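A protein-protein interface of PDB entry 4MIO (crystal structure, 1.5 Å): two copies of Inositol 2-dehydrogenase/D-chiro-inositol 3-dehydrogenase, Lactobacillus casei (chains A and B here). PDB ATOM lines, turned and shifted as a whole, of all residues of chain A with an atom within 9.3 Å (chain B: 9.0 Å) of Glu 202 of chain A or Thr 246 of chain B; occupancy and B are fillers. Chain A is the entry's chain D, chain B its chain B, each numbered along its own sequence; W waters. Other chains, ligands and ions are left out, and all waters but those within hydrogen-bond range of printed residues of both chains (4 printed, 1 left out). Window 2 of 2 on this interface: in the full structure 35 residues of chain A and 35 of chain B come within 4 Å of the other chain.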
ATOM      1  N   ILE A 156      27.305  -7.974 -30.128  1.00  0.00           N
ATOM      2  CA  ILE A 156      26.057  -7.871 -29.421  1.00  0.00           C
ATOM      3  C   ILE A 156      26.296  -7.612 -27.925  1.00  0.00           C
ATOM      4  O   ILE A 156      27.053  -8.277 -27.332  1.00  0.00           O
ATOM      5  CB  ILE A 156      25.276  -9.185 -29.520  1.00  0.00           C
ATOM      6  CG1 ILE A 156      25.091  -9.634 -30.965  1.00  0.00           C
ATOM      7  CG2 ILE A 156      23.970  -9.049 -28.812  1.00  0.00           C
ATOM      8  CD1 ILE A 156      24.378  -8.679 -31.858  1.00  0.00           C
ATOM      9  N   ASN A 157      25.614  -6.607 -27.383  1.00  0.00           N
ATOM     10  CA  ASN A 157      25.618  -6.347 -25.954  1.00  0.00           C
ATOM     11  C   ASN A 157      24.158  -6.271 -25.505  1.00  0.00           C
ATOM     12  O   ASN A 157      23.332  -5.915 -26.255  1.00  0.00           O
ATOM     13  CB  ASN A 157      26.215  -4.987 -25.596  1.00  0.00           C
ATOM     14  CG  ASN A 157      27.661  -4.803 -25.955  1.00  0.00           C
ATOM     15  OD1 ASN A 157      28.137  -3.721 -25.851  1.00  0.00           O
ATOM     16  ND2 ASN A 157      28.339  -5.827 -26.355  1.00  0.00           N
ATOM     17  N   PRO A 158      23.894  -6.588 -24.237  1.00  0.00           N
ATOM     18  CA  PRO A 158      22.506  -6.596 -23.804  1.00  0.00           C
ATOM     19  C   PRO A 158      21.936  -5.193 -23.574  1.00  0.00           C
ATOM     20  O   PRO A 158      20.829  -4.914 -23.864  1.00  0.00           O
ATOM     21  CB  PRO A 158      22.562  -7.397 -22.505  1.00  0.00           C
ATOM     22  CG  PRO A 158      23.910  -7.363 -22.083  1.00  0.00           C
ATOM     23  CD  PRO A 158      24.766  -7.246 -23.268  1.00  0.00           C
ATOM     24  N   ASN A 159      22.785  -4.355 -23.026  1.00  0.00           N
ATOM     25  CA  ASN A 159      22.443  -2.988 -22.739  1.00  0.00           C
ATOM     26  C   ASN A 159      23.695  -2.146 -22.520  1.00  0.00           C
ATOM     27  O   ASN A 159      24.739  -2.674 -22.469  1.00  0.00           O
ATOM     28  CB  ASN A 159      21.536  -2.908 -21.537  1.00  0.00           C
ATOM     29  CG  ASN A 159      22.051  -3.729 -20.407  1.00  0.00           C
ATOM     30  OD1 ASN A 159      23.112  -3.470 -19.905  1.00  0.00           O
ATOM     31  ND2 ASN A 159      21.310  -4.749 -20.021  1.00  0.00           N
ATOM     32  N   VAL A 160      23.523  -0.854 -22.432  1.00  0.00           N
ATOM     33  CA  VAL A 160      24.636   0.028 -22.193  1.00  0.00           C
ATOM     34  C   VAL A 160      24.357   0.951 -20.982  1.00  0.00           C
ATOM     35  O   VAL A 160      23.249   1.196 -20.644  1.00  0.00           O
ATOM     36  CB  VAL A 160      25.005   0.894 -23.432  1.00  0.00           C
ATOM     37  CG1 VAL A 160      25.465   0.055 -24.555  1.00  0.00           C
ATOM     38  CG2 VAL A 160      23.859   1.779 -23.872  1.00  0.00           C
ATOM     39  N   ARG A 198      16.166   0.486 -38.603  1.00  0.00           N
ATOM     40  CA  ARG A 198      15.075   0.773 -37.708  1.00  0.00           C
ATOM     41  C   ARG A 198      15.563   0.923 -36.262  1.00  0.00           C
ATOM     42  O   ARG A 198      16.119   0.018 -35.735  1.00  0.00           O
ATOM     43  CB  ARG A 198      14.072  -0.382 -37.812  1.00  0.00           C
ATOM     44  CG  ARG A 198      12.754  -0.177 -37.137  1.00  0.00           C
ATOM     45  CD  ARG A 198      11.866  -1.410 -37.346  1.00  0.00           C
ATOM     46  NE  ARG A 198      10.522  -1.268 -36.827  1.00  0.00           N
ATOM     47  CZ  ARG A 198       9.582  -2.190 -36.958  1.00  0.00           C
ATOM     48  NH1 ARG A 198       9.837  -3.339 -37.544  1.00  0.00           N
ATOM     49  NH2 ARG A 198       8.381  -1.962 -36.490  1.00  0.00           N
ATOM     50  N   GLN A 199      15.344   2.093 -35.682  1.00  0.00           N
ATOM     51  CA  GLN A 199      15.768   2.369 -34.321  1.00  0.00           C
ATOM     52  C   GLN A 199      15.034   1.490 -33.311  1.00  0.00           C
ATOM     53  O   GLN A 199      13.862   1.391 -33.322  1.00  0.00           O
ATOM     54  CB  GLN A 199      15.552   3.835 -33.982  1.00  0.00           C
ATOM     55  CG  GLN A 199      15.779   4.186 -32.529  1.00  0.00           C
ATOM     56  CD  GLN A 199      17.250   4.367 -32.176  1.00  0.00           C
ATOM     57  OE1 GLN A 199      18.116   4.013 -32.938  1.00  0.00           O
ATOM     58  NE2 GLN A 199      17.500   4.953 -31.029  1.00  0.00           N
ATOM     59  N   SER A 200      15.790   0.871 -32.428  1.00  0.00           N
ATOM     60  CA  SER A 200      15.200   0.049 -31.394  1.00  0.00           C
ATOM     61  C   SER A 200      14.464   0.841 -30.305  1.00  0.00           C
ATOM     62  O   SER A 200      14.930   1.836 -29.846  1.00  0.00           O
ATOM     63  CB  SER A 200      16.275  -0.785 -30.694  1.00  0.00           C
ATOM     64  OG  SER A 200      15.694  -1.591 -29.725  1.00  0.00           O
ATOM     65  N   ALA A 201      13.317   0.326 -29.917  1.00  0.00           N
ATOM     66  CA  ALA A 201      12.588   0.886 -28.798  1.00  0.00           C
ATOM     67  C   ALA A 201      13.305   0.692 -27.473  1.00  0.00           C
ATOM     68  O   ALA A 201      12.918   1.257 -26.486  1.00  0.00           O
ATOM     69  CB  ALA A 201      11.208   0.267 -28.708  1.00  0.00           C
ATOM     70  N   GLU A 202      14.353  -0.126 -27.472  1.00  0.00           N
ATOM     71  CA  GLU A 202      15.086  -0.400 -26.260  1.00  0.00           C
ATOM     72  C   GLU A 202      16.164   0.634 -25.895  1.00  0.00           C
ATOM     73  O   GLU A 202      16.690   0.578 -24.825  1.00  0.00           O
ATOM     74  CB  GLU A 202      15.714  -1.775 -26.297  1.00  0.00           C
ATOM     75  CG  GLU A 202      14.752  -2.921 -26.443  1.00  0.00           C
ATOM     76  CD  GLU A 202      13.717  -3.027 -25.350  1.00  0.00           C
ATOM     77  OE1 GLU A 202      12.542  -3.188 -25.651  1.00  0.00           O
ATOM     78  OE2 GLU A 202      14.074  -2.970 -24.217  1.00  0.00           O
ATOM     79  N   VAL A 203      16.440   1.544 -26.797  1.00  0.00           N
ATOM     80  CA  VAL A 203      17.416   2.578 -26.565  1.00  0.00           C
ATOM     81  C   VAL A 203      16.935   3.542 -25.477  1.00  0.00           C
ATOM     82  O   VAL A 203      15.826   3.979 -25.513  1.00  0.00           O
ATOM     83  CB  VAL A 203      17.739   3.344 -27.823  1.00  0.00           C
ATOM     84  CG1 VAL A 203      18.620   4.546 -27.525  1.00  0.00           C
ATOM     85  CG2 VAL A 203      18.424   2.429 -28.824  1.00  0.00           C
ATOM     86  N   ARG A 204      17.815   3.828 -24.537  1.00  0.00           N
ATOM     87  CA  ARG A 204      17.514   4.677 -23.400  1.00  0.00           C
ATOM     88  C   ARG A 204      18.479   5.873 -23.293  1.00  0.00           C
ATOM     89  O   ARG A 204      18.466   6.581 -22.330  1.00  0.00           O
ATOM     90  CB  ARG A 204      17.617   3.863 -22.129  1.00  0.00           C
ATOM     91  CG  ARG A 204      16.561   2.814 -21.967  1.00  0.00           C
ATOM     92  CD  ARG A 204      16.938   1.895 -20.875  1.00  0.00           C
ATOM     93  NE  ARG A 204      17.806   2.558 -19.923  1.00  0.00           N
ATOM     94  CZ  ARG A 204      17.439   3.063 -18.766  1.00  0.00           C
ATOM     95  NH1 ARG A 204      16.186   2.999 -18.377  1.00  0.00           N
ATOM     96  NH2 ARG A 204      18.330   3.644 -18.012  1.00  0.00           N
ATOM     97  N   ASN A 205      19.324   6.016 -24.289  1.00  0.00           N
ATOM     98  CA  ASN A 205      20.335   7.035 -24.293  1.00  0.00           C
ATOM     99  C   ASN A 205      20.107   8.042 -25.404  1.00  0.00           C
ATOM    100  O   ASN A 205      20.073   7.688 -26.544  1.00  0.00           O
ATOM    101  CB  ASN A 205      21.739   6.418 -24.490  1.00  0.00           C
ATOM    102  CG  ASN A 205      22.181   5.538 -23.333  1.00  0.00           C
ATOM    103  OD1 ASN A 205      21.393   4.912 -22.680  1.00  0.00           O
ATOM    104  ND2 ASN A 205      23.432   5.480 -23.132  1.00  0.00           N
ATOM    105  N   LEU A 208      21.757   8.096 -29.180  1.00  0.00           N
ATOM    106  CA  LEU A 208      22.262   6.811 -29.563  1.00  0.00           C
ATOM    107  C   LEU A 208      21.381   6.133 -30.625  1.00  0.00           C
ATOM    108  O   LEU A 208      20.228   5.950 -30.422  1.00  0.00           O
ATOM    109  CB  LEU A 208      22.388   5.874 -28.352  1.00  0.00           C
ATOM    110  CG  LEU A 208      22.845   4.438 -28.599  1.00  0.00           C
ATOM    111  CD1 LEU A 208      24.235   4.383 -29.232  1.00  0.00           C
ATOM    112  CD2 LEU A 208      22.836   3.644 -27.314  1.00  0.00           C
ATOM    113  N   HIS A 209      22.006   5.781 -31.734  1.00  0.00           N
ATOM    114  CA  HIS A 209      21.366   4.948 -32.751  1.00  0.00           C
ATOM    115  C   HIS A 209      21.753   3.512 -32.521  1.00  0.00           C
ATOM    116  O   HIS A 209      22.881   3.216 -32.369  1.00  0.00           O
ATOM    117  CB  HIS A 209      21.822   5.366 -34.150  1.00  0.00           C
ATOM    118  CG  HIS A 209      21.411   6.742 -34.559  1.00  0.00           C
ATOM    119  ND1 HIS A 209      20.301   6.991 -35.315  1.00  0.00           N
ATOM    120  CD2 HIS A 209      21.976   7.939 -34.321  1.00  0.00           C
ATOM    121  CE1 HIS A 209      20.204   8.285 -35.529  1.00  0.00           C
ATOM    122  NE2 HIS A 209      21.206   8.883 -34.934  1.00  0.00           N
ATOM    123  N   ASP A 210      20.760   2.636 -32.484  1.00  0.00           N
ATOM    124  CA  ASP A 210      21.004   1.223 -32.258  1.00  0.00           C
ATOM    125  C   ASP A 210      19.855   0.438 -32.851  1.00  0.00           C
ATOM    126  O   ASP A 210      18.756   0.768 -32.601  1.00  0.00           O
ATOM    127  CB  ASP A 210      21.127   0.903 -30.770  1.00  0.00           C
ATOM    128  CG  ASP A 210      21.688  -0.489 -30.497  1.00  0.00           C
ATOM    129  OD1 ASP A 210      22.763  -0.797 -30.988  1.00  0.00           O
ATOM    130  OD2 ASP A 210      21.024  -1.226 -29.791  1.00  0.00           O
ATOM    131  N   PRO A 211      20.162  -0.594 -33.636  1.00  0.00           N
ATOM    132  CA  PRO A 211      21.490  -1.072 -34.002  1.00  0.00           C
ATOM    133  C   PRO A 211      22.178  -0.195 -35.052  1.00  0.00           C
ATOM    134  O   PRO A 211      21.620   0.729 -35.521  1.00  0.00           O
ATOM    135  CB  PRO A 211      21.213  -2.471 -34.541  1.00  0.00           C
ATOM    136  CG  PRO A 211      19.853  -2.447 -34.982  1.00  0.00           C
ATOM    137  CD  PRO A 211      19.118  -1.531 -34.076  1.00  0.00           C
ATOM    138  N   HIS A 229      24.955  -4.179 -32.124  1.00  0.00           N
ATOM    139  CA  HIS A 229      23.662  -4.116 -31.478  1.00  0.00           C
ATOM    140  C   HIS A 229      23.863  -4.157 -29.961  1.00  0.00           C
ATOM    141  O   HIS A 229      24.091  -5.180 -29.409  1.00  0.00           O
ATOM    142  CB  HIS A 229      22.772  -5.263 -31.928  1.00  0.00           C
ATOM    143  CG  HIS A 229      21.334  -5.119 -31.535  1.00  0.00           C
ATOM    144  ND1 HIS A 229      20.426  -6.131 -31.679  1.00  0.00           N
ATOM    145  CD2 HIS A 229      20.649  -4.083 -31.030  1.00  0.00           C
ATOM    146  CE1 HIS A 229      19.246  -5.712 -31.282  1.00  0.00           C
ATOM    147  NE2 HIS A 229      19.363  -4.482 -30.861  1.00  0.00           N
ATOM    148  N   VAL A 230      23.795  -2.990 -29.345  1.00  0.00           N
ATOM    149  CA  VAL A 230      24.201  -2.839 -27.966  1.00  0.00           C
ATOM    150  C   VAL A 230      23.070  -2.736 -26.931  1.00  0.00           C
ATOM    151  O   VAL A 230      23.351  -2.679 -25.764  1.00  0.00           O
ATOM    152  CB  VAL A 230      25.205  -1.691 -27.791  1.00  0.00           C
ATOM    153  CG1 VAL A 230      26.376  -1.914 -28.692  1.00  0.00           C
ATOM    154  CG2 VAL A 230      24.588  -0.355 -28.087  1.00  0.00           C
ATOM    155  N   THR A 231      21.829  -2.777 -27.405  1.00  0.00           N
ATOM    156  CA  THR A 231      20.660  -2.853 -26.540  1.00  0.00           C
ATOM    157  C   THR A 231      19.856  -4.096 -26.856  1.00  0.00           C
ATOM    158  O   THR A 231      18.673  -4.100 -26.743  1.00  0.00           O
ATOM    159  CB  THR A 231      19.732  -1.633 -26.635  1.00  0.00           C
ATOM    160  OG1 THR A 231      19.131  -1.578 -27.927  1.00  0.00           O
ATOM    161  CG2 THR A 231      20.526  -0.348 -26.371  1.00  0.00           C
ATOM    162  N   ALA A 232      20.572  -5.151 -27.226  1.00  0.00           N
ATOM    163  CA  ALA A 232      19.961  -6.412 -27.658  1.00  0.00           C
ATOM    164  C   ALA A 232      19.132  -7.190 -26.632  1.00  0.00           C
ATOM    165  O   ALA A 232      18.413  -8.053 -27.002  1.00  0.00           O
ATOM    166  CB  ALA A 232      21.023  -7.329 -28.256  1.00  0.00           C
ATOM    167  N   GLN A 233      19.305  -6.851 -25.368  1.00  0.00           N
ATOM    168  CA  GLN A 233      18.624  -7.455 -24.221  1.00  0.00           C
ATOM    169  C   GLN A 233      19.032  -8.905 -23.861  1.00  0.00           C
ATOM    170  O   GLN A 233      19.207  -9.234 -22.736  1.00  0.00           O
ATOM    171  CB  GLN A 233      17.109  -7.365 -24.331  1.00  0.00           C
ATOM    172  CG  GLN A 233      16.563  -5.986 -24.600  1.00  0.00           C
ATOM    173  CD  GLN A 233      17.024  -4.984 -23.545  1.00  0.00           C
ATOM    174  OE1 GLN A 233      16.815  -5.190 -22.386  1.00  0.00           O
ATOM    175  NE2 GLN A 233      17.671  -3.925 -23.985  1.00  0.00           N
ATOM    176  N   TYR A 234      19.149  -9.745 -24.871  1.00  0.00           N
ATOM    177  CA  TYR A 234      19.212 -11.162 -24.606  1.00  0.00           C
ATOM    178  C   TYR A 234      20.538 -11.669 -24.013  1.00  0.00           C
ATOM    179  O   TYR A 234      20.583 -12.668 -23.372  1.00  0.00           O
ATOM    180  CB  TYR A 234      18.873 -11.990 -25.883  1.00  0.00           C
ATOM    181  CG  TYR A 234      20.004 -12.160 -26.889  1.00  0.00           C
ATOM    182  CD1 TYR A 234      20.919 -13.156 -26.780  1.00  0.00           C
ATOM    183  CD2 TYR A 234      20.115 -11.318 -27.953  1.00  0.00           C
ATOM    184  CE1 TYR A 234      21.929 -13.282 -27.685  1.00  0.00           C
ATOM    185  CE2 TYR A 234      21.110 -11.449 -28.861  1.00  0.00           C
ATOM    186  CZ  TYR A 234      22.007 -12.421 -28.724  1.00  0.00           C
ATOM    187  OH  TYR A 234      23.008 -12.551 -29.632  1.00  0.00           O
ATOM    188  N   GLY A 235      21.596 -10.936 -24.296  1.00  0.00           N
ATOM    189  CA  GLY A 235      22.897 -11.420 -23.945  1.00  0.00           C
ATOM    190  C   GLY A 235      24.037 -10.653 -24.599  1.00  0.00           C
ATOM    191  O   GLY A 235      23.809  -9.714 -25.304  1.00  0.00           O
ATOM    192  N   GLY B 143       5.752 -11.800 -31.120  1.00  0.00           N
ATOM    193  CA  GLY B 143       6.291 -10.645 -30.447  1.00  0.00           C
ATOM    194  C   GLY B 143       7.456 -10.892 -29.486  1.00  0.00           C
ATOM    195  O   GLY B 143       7.933  -9.998 -28.878  1.00  0.00           O
ATOM    196  N   ILE B 144       7.875 -12.130 -29.414  1.00  0.00           N
ATOM    197  CA  ILE B 144       8.833 -12.540 -28.431  1.00  0.00           C
ATOM    198  C   ILE B 144      10.226 -11.859 -28.526  1.00  0.00           C
ATOM    199  O   ILE B 144      10.890 -11.732 -27.555  1.00  0.00           O
ATOM    200  CB  ILE B 144       8.968 -14.074 -28.361  1.00  0.00           C
ATOM    201  CG1 ILE B 144       9.693 -14.512 -27.094  1.00  0.00           C
ATOM    202  CG2 ILE B 144       9.611 -14.630 -29.613  1.00  0.00           C
ATOM    203  CD1 ILE B 144       9.519 -15.944 -26.788  1.00  0.00           C
ATOM    204  N   ILE B 145      10.594 -11.449 -29.713  1.00  0.00           N
ATOM    205  CA  ILE B 145      11.838 -10.727 -29.890  1.00  0.00           C
ATOM    206  C   ILE B 145      11.632  -9.262 -30.217  1.00  0.00           C
ATOM    207  O   ILE B 145      12.527  -8.569 -30.559  1.00  0.00           O
ATOM    208  CB  ILE B 145      12.818 -11.417 -30.928  1.00  0.00           C
ATOM    209  CG1 ILE B 145      12.288 -11.386 -32.366  1.00  0.00           C
ATOM    210  CG2 ILE B 145      13.106 -12.803 -30.532  1.00  0.00           C
ATOM    211  CD1 ILE B 145      13.341 -11.653 -33.386  1.00  0.00           C
ATOM    212  N   GLY B 146      10.409  -8.813 -30.029  1.00  0.00           N
ATOM    213  CA  GLY B 146      10.097  -7.445 -30.360  1.00  0.00           C
ATOM    214  C   GLY B 146      10.108  -7.211 -31.862  1.00  0.00           C
ATOM    215  O   GLY B 146      10.006  -8.112 -32.612  1.00  0.00           O
ATOM    216  N   ALA B 147      10.218  -5.964 -32.248  1.00  0.00           N
ATOM    217  CA  ALA B 147      10.170  -5.617 -33.648  1.00  0.00           C
ATOM    218  C   ALA B 147      11.451  -6.024 -34.404  1.00  0.00           C
ATOM    219  O   ALA B 147      12.509  -5.932 -33.889  1.00  0.00           O
ATOM    220  CB  ALA B 147       9.935  -4.128 -33.792  1.00  0.00           C
ATOM    221  N   PRO B 148      11.288  -6.472 -35.650  1.00  0.00           N
ATOM    222  CA  PRO B 148      12.457  -6.843 -36.448  1.00  0.00           C
ATOM    223  C   PRO B 148      13.183  -5.618 -37.019  1.00  0.00           C
ATOM    224  O   PRO B 148      12.598  -4.813 -37.673  1.00  0.00           O
ATOM    225  CB  PRO B 148      11.852  -7.706 -37.554  1.00  0.00           C
ATOM    226  CG  PRO B 148      10.473  -7.161 -37.715  1.00  0.00           C
ATOM    227  CD  PRO B 148      10.032  -6.783 -36.329  1.00  0.00           C
ATOM    228  N   LEU B 149      14.460  -5.536 -36.700  1.00  0.00           N
ATOM    229  CA  LEU B 149      15.283  -4.374 -37.030  1.00  0.00           C
ATOM    230  C   LEU B 149      16.208  -4.638 -38.228  1.00  0.00           C
ATOM    231  O   LEU B 149      16.385  -3.810 -39.041  1.00  0.00           O
ATOM    232  CB  LEU B 149      16.096  -3.964 -35.813  1.00  0.00           C
ATOM    233  CG  LEU B 149      15.315  -3.852 -34.519  1.00  0.00           C
ATOM    234  CD1 LEU B 149      16.234  -3.537 -33.351  1.00  0.00           C
ATOM    235  CD2 LEU B 149      14.228  -2.778 -34.677  1.00  0.00           C
ATOM    236  N   VAL B 242      16.794 -13.175 -37.973  1.00  0.00           N
ATOM    237  CA  VAL B 242      16.080 -11.966 -37.708  1.00  0.00           C
ATOM    238  C   VAL B 242      16.536 -11.398 -36.381  1.00  0.00           C
ATOM    239  O   VAL B 242      16.549 -12.039 -35.428  1.00  0.00           O
ATOM    240  CB  VAL B 242      14.572 -12.173 -37.710  1.00  0.00           C
ATOM    241  CG1 VAL B 242      13.851 -10.876 -37.391  1.00  0.00           C
ATOM    242  CG2 VAL B 242      14.134 -12.759 -39.052  1.00  0.00           C
ATOM    243  N   ILE B 243      16.944 -10.166 -36.432  1.00  0.00           N
ATOM    244  CA  ILE B 243      17.430  -9.421 -35.279  1.00  0.00           C
ATOM    245  C   ILE B 243      16.325  -8.499 -34.782  1.00  0.00           C
ATOM    246  O   ILE B 243      15.934  -7.614 -35.433  1.00  0.00           O
ATOM    247  CB  ILE B 243      18.583  -8.507 -35.700  1.00  0.00           C
ATOM    248  CG1 ILE B 243      19.649  -9.275 -36.442  1.00  0.00           C
ATOM    249  CG2 ILE B 243      19.110  -7.741 -34.495  1.00  0.00           C
ATOM    250  CD1 ILE B 243      20.321 -10.318 -35.651  1.00  0.00           C
ATOM    251  N   GLY B 244      15.881  -8.806 -33.584  1.00  0.00           N
ATOM    252  CA  GLY B 244      14.848  -8.076 -32.946  1.00  0.00           C
ATOM    253  C   GLY B 244      15.337  -7.170 -31.856  1.00  0.00           C
ATOM    254  O   GLY B 244      16.409  -7.215 -31.467  1.00  0.00           O
ATOM    255  N   GLU B 245      14.419  -6.366 -31.399  1.00  0.00           N
ATOM    256  CA  GLU B 245      14.666  -5.454 -30.317  1.00  0.00           C
ATOM    257  C   GLU B 245      15.156  -6.157 -29.040  1.00  0.00           C
ATOM    258  O   GLU B 245      15.997  -5.652 -28.377  1.00  0.00           O
ATOM    259  CB  GLU B 245      13.407  -4.646 -30.009  1.00  0.00           C
ATOM    260  CG  GLU B 245      13.070  -3.612 -31.070  1.00  0.00           C
ATOM    261  CD  GLU B 245      11.731  -2.954 -30.848  1.00  0.00           C
ATOM    262  OE1 GLU B 245      10.823  -3.640 -30.437  1.00  0.00           O
ATOM    263  OE2 GLU B 245      11.636  -1.766 -31.129  1.00  0.00           O
ATOM    264  N   THR B 246      14.573  -7.311 -28.746  1.00  0.00           N
ATOM    265  CA  THR B 246      14.821  -8.003 -27.511  1.00  0.00           C
ATOM    266  C   THR B 246      15.361  -9.435 -27.650  1.00  0.00           C
ATOM    267  O   THR B 246      15.535 -10.104 -26.700  1.00  0.00           O
ATOM    268  CB  THR B 246      13.587  -8.052 -26.625  1.00  0.00           C
ATOM    269  OG1 THR B 246      12.632  -8.928 -27.199  1.00  0.00           O
ATOM    270  CG2 THR B 246      12.993  -6.662 -26.458  1.00  0.00           C
ATOM    271  N   GLY B 247      15.625  -9.846 -28.874  1.00  0.00           N
ATOM    272  CA  GLY B 247      16.211 -11.123 -29.103  1.00  0.00           C
ATOM    273  C   GLY B 247      16.430 -11.382 -30.593  1.00  0.00           C
ATOM    274  O   GLY B 247      16.259 -10.517 -31.369  1.00  0.00           O
ATOM    275  N   GLU B 248      16.833 -12.597 -30.910  1.00  0.00           N
ATOM    276  CA  GLU B 248      17.046 -13.012 -32.289  1.00  0.00           C
ATOM    277  C   GLU B 248      16.380 -14.358 -32.576  1.00  0.00           C
ATOM    278  O   GLU B 248      16.178 -15.139 -31.698  1.00  0.00           O
ATOM    279  CB  GLU B 248      18.542 -13.130 -32.617  1.00  0.00           C
ATOM    280  CG  GLU B 248      19.378 -11.912 -32.306  1.00  0.00           C
ATOM    281  CD  GLU B 248      20.839 -12.067 -32.730  1.00  0.00           C
ATOM    282  OE1 GLU B 248      21.180 -13.156 -33.135  1.00  0.00           O
ATOM    283  OE2 GLU B 248      21.596 -11.087 -32.651  1.00  0.00           O
ATOM    284  N   LEU B 249      16.098 -14.574 -33.853  1.00  0.00           N
ATOM    285  CA  LEU B 249      15.585 -15.837 -34.346  1.00  0.00           C
ATOM    286  C   LEU B 249      16.415 -16.301 -35.550  1.00  0.00           C
ATOM    287  O   LEU B 249      16.709 -15.513 -36.387  1.00  0.00           O
ATOM    288  CB  LEU B 249      14.122 -15.711 -34.752  1.00  0.00           C
ATOM    289  CG  LEU B 249      13.109 -15.593 -33.611  1.00  0.00           C
ATOM    290  CD1 LEU B 249      11.796 -15.097 -34.118  1.00  0.00           C
ATOM    291  CD2 LEU B 249      12.948 -16.897 -32.904  1.00  0.00           C
HETATM  292  O   HOH W   1      17.384  -3.454 -29.131  1.00  0.00           O
HETATM  293  O   HOH W   2      10.637  -4.275 -27.707  1.00  0.00           O
HETATM  294  O   HOH W   3      20.683  -8.950 -31.531  1.00  0.00           O
HETATM  295  O   HOH W   4      11.632  -0.183 -33.277  1.00  0.00           O
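The backbone carbonyl oxygen of Pro 148 of chain B is in hydrogen-bond range of the guanidinium group of Arg 198 of chain A (3.1 Å).
OE2 of Glu 245 of chain B lies within hydrogen-bond range of N of Ala 201 of chain A (2.9 Å).
O of Glu 245 of chain B lies close to O of Thr 231 of chain A (3.5 Å).
The backbone NH (N) of Glu 245 of chain B is in hydrogen-bond range of the backbone carbonyl oxygen (O) of Ile 145 of chain B.
O of Ile 145 of chain B is in hydrogen-bond range of N of Thr 246 of chain B.
The backbone NH of Leu 149 of chain B is in hydrogen-bond range of the backbone carbonyl oxygen of Ile 243 of chain B, 2.8 Å away.
The backbone NH (N) of Ala 232 of chain A sits at hydrogen-bond distance from the backbone carbonyl oxygen (O) of Pro 158 of chain A (3.4 Å).
Among the printed residues, pairs that only touch across the chains: His 229 of chain A with Gly 244 of chain B (3.2 Å), Ala 232 of chain A with Thr 246 of chain B (3.4 Å), His 229 of chain A with Ile 243 of chain B (3.5 Å), Arg 198 of chain A with Leu 149 of chain B (3.5 Å), Glu 202 of chain A with Glu 245 of chain B (3.6 Å), Ser 200 of chain A with Glu 245 of chain B (3.6 Å), Pro 211 of chain A with Leu 149 of chain B (3.6 Å), Glu 202 of chain A with Thr 246 of chain B (3.6 Å), Tyr 234 of chain A with Glu 248 of chain B (3.6 Å), Ala 232 of chain A with Glu 245 of chain B (3.7 Å), Arg 198 of chain A with Ala 147 of chain B (3.7 Å), Ile 156 of chain A with Glu 248 of chain B (3.8 Å), Ala 232 of chain A with Gly 247 of chain B (3.8 Å), Ser 200 of chain A with Leu 149 of chain B (3.8 Å), Gln 233 of chain A with Glu 245 of chain B (3.8 Å), Tyr 234 of chain A with Thr 246 of chain B (3.9 Å) and Gln 233 of chain A with Thr 246 of chain B (3.9 Å).
Asn 159 of chain A touches none of the printed residues of chain B.
Of the printed residues of chain B, Ser 200 of chain A touches Leu 149 (3.8 Å) and Glu 245 (3.6 Å).
Of the printed residues of chain B, Ala 201 of chain A touches Glu 245.
Of chain B, only Glu 245 (3.6 Å) and Thr 246 (3.6 Å) come within 4 Å of Glu 202 of chain A.
Val 203 of chain A touches none of the printed residues of chain B.
Of the printed residues of chain B, His 229 of chain A touches Ile 243 and Gly 244.
Of the printed residues of chain A, Ala 147 of chain B touches Arg 198.
Of the printed residues of chain A, Ile 243 of chain B touches His 229.
Glu 245 of chain B touches just these residues of chain A: Ser 200 (3.6 Å), Ala 201 (2.9 Å), Glu 202 (3.6 Å), Thr 231 (3.5 Å), Ala 232 (3.7 Å) and Gln 233 (3.8 Å).
Gly 247 of chain B touches just one residue of chain A: Ala 232 (3.8 Å).
The nearest printed residue of chain A that does not touch Thr 246 of chain B is Thr 231 of chain A (5.5 Å).
Hydrophobic or aromatic side chains of chain A within 4 Å of the printed part of chain B: Ile 156, Ala 201, Pro 211, His 229 and Tyr 234.
Of the 15 printed residues of chain B, 9 touch a printed residue of chain A.
Hydrophobic or aromatic side chains of chain B that line the printed part of chain A: Ala 147, Pro 148, Leu 149 and Ile 243.
Among the printed residues, 20 pairs touch across the chains.
Among the printed residues, no Asp or Glu carboxylate lies within 4 Å of a Lys or Arg side-chain nitrogen of the other chain.
No position is printed for both chains.
Of the 20 pairs that touch across the chains among the printed residues, none has its exchanged pair printed and touching as well.
Water W3 lies within hydrogen-bond range of OE2 of Glu 248 of chain B (2.6 Å) and ND1 of His 229 of chain A (2.8 Å).
Water W1 lies within hydrogen-bond range of OG of Ser 200 of chain A (2.6 Å), O of Glu 245 of chain B (2.7 Å), O of Thr 231 of chain A (2.8 Å) and NE2 of His 229 of chain A (2.8 Å).
Water W4 bridges the side-chain carboxylate (OE2) of Glu 245 of chain B (2.7 Å) and the backbone carbonyl oxygen (O) of Gln 199 of chain A (2.7 Å).
Water W2 bridges OE1 of Glu 245 of chain B (2.8 Å) and OE1 of Glu 202 of chain A (3.0 Å).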
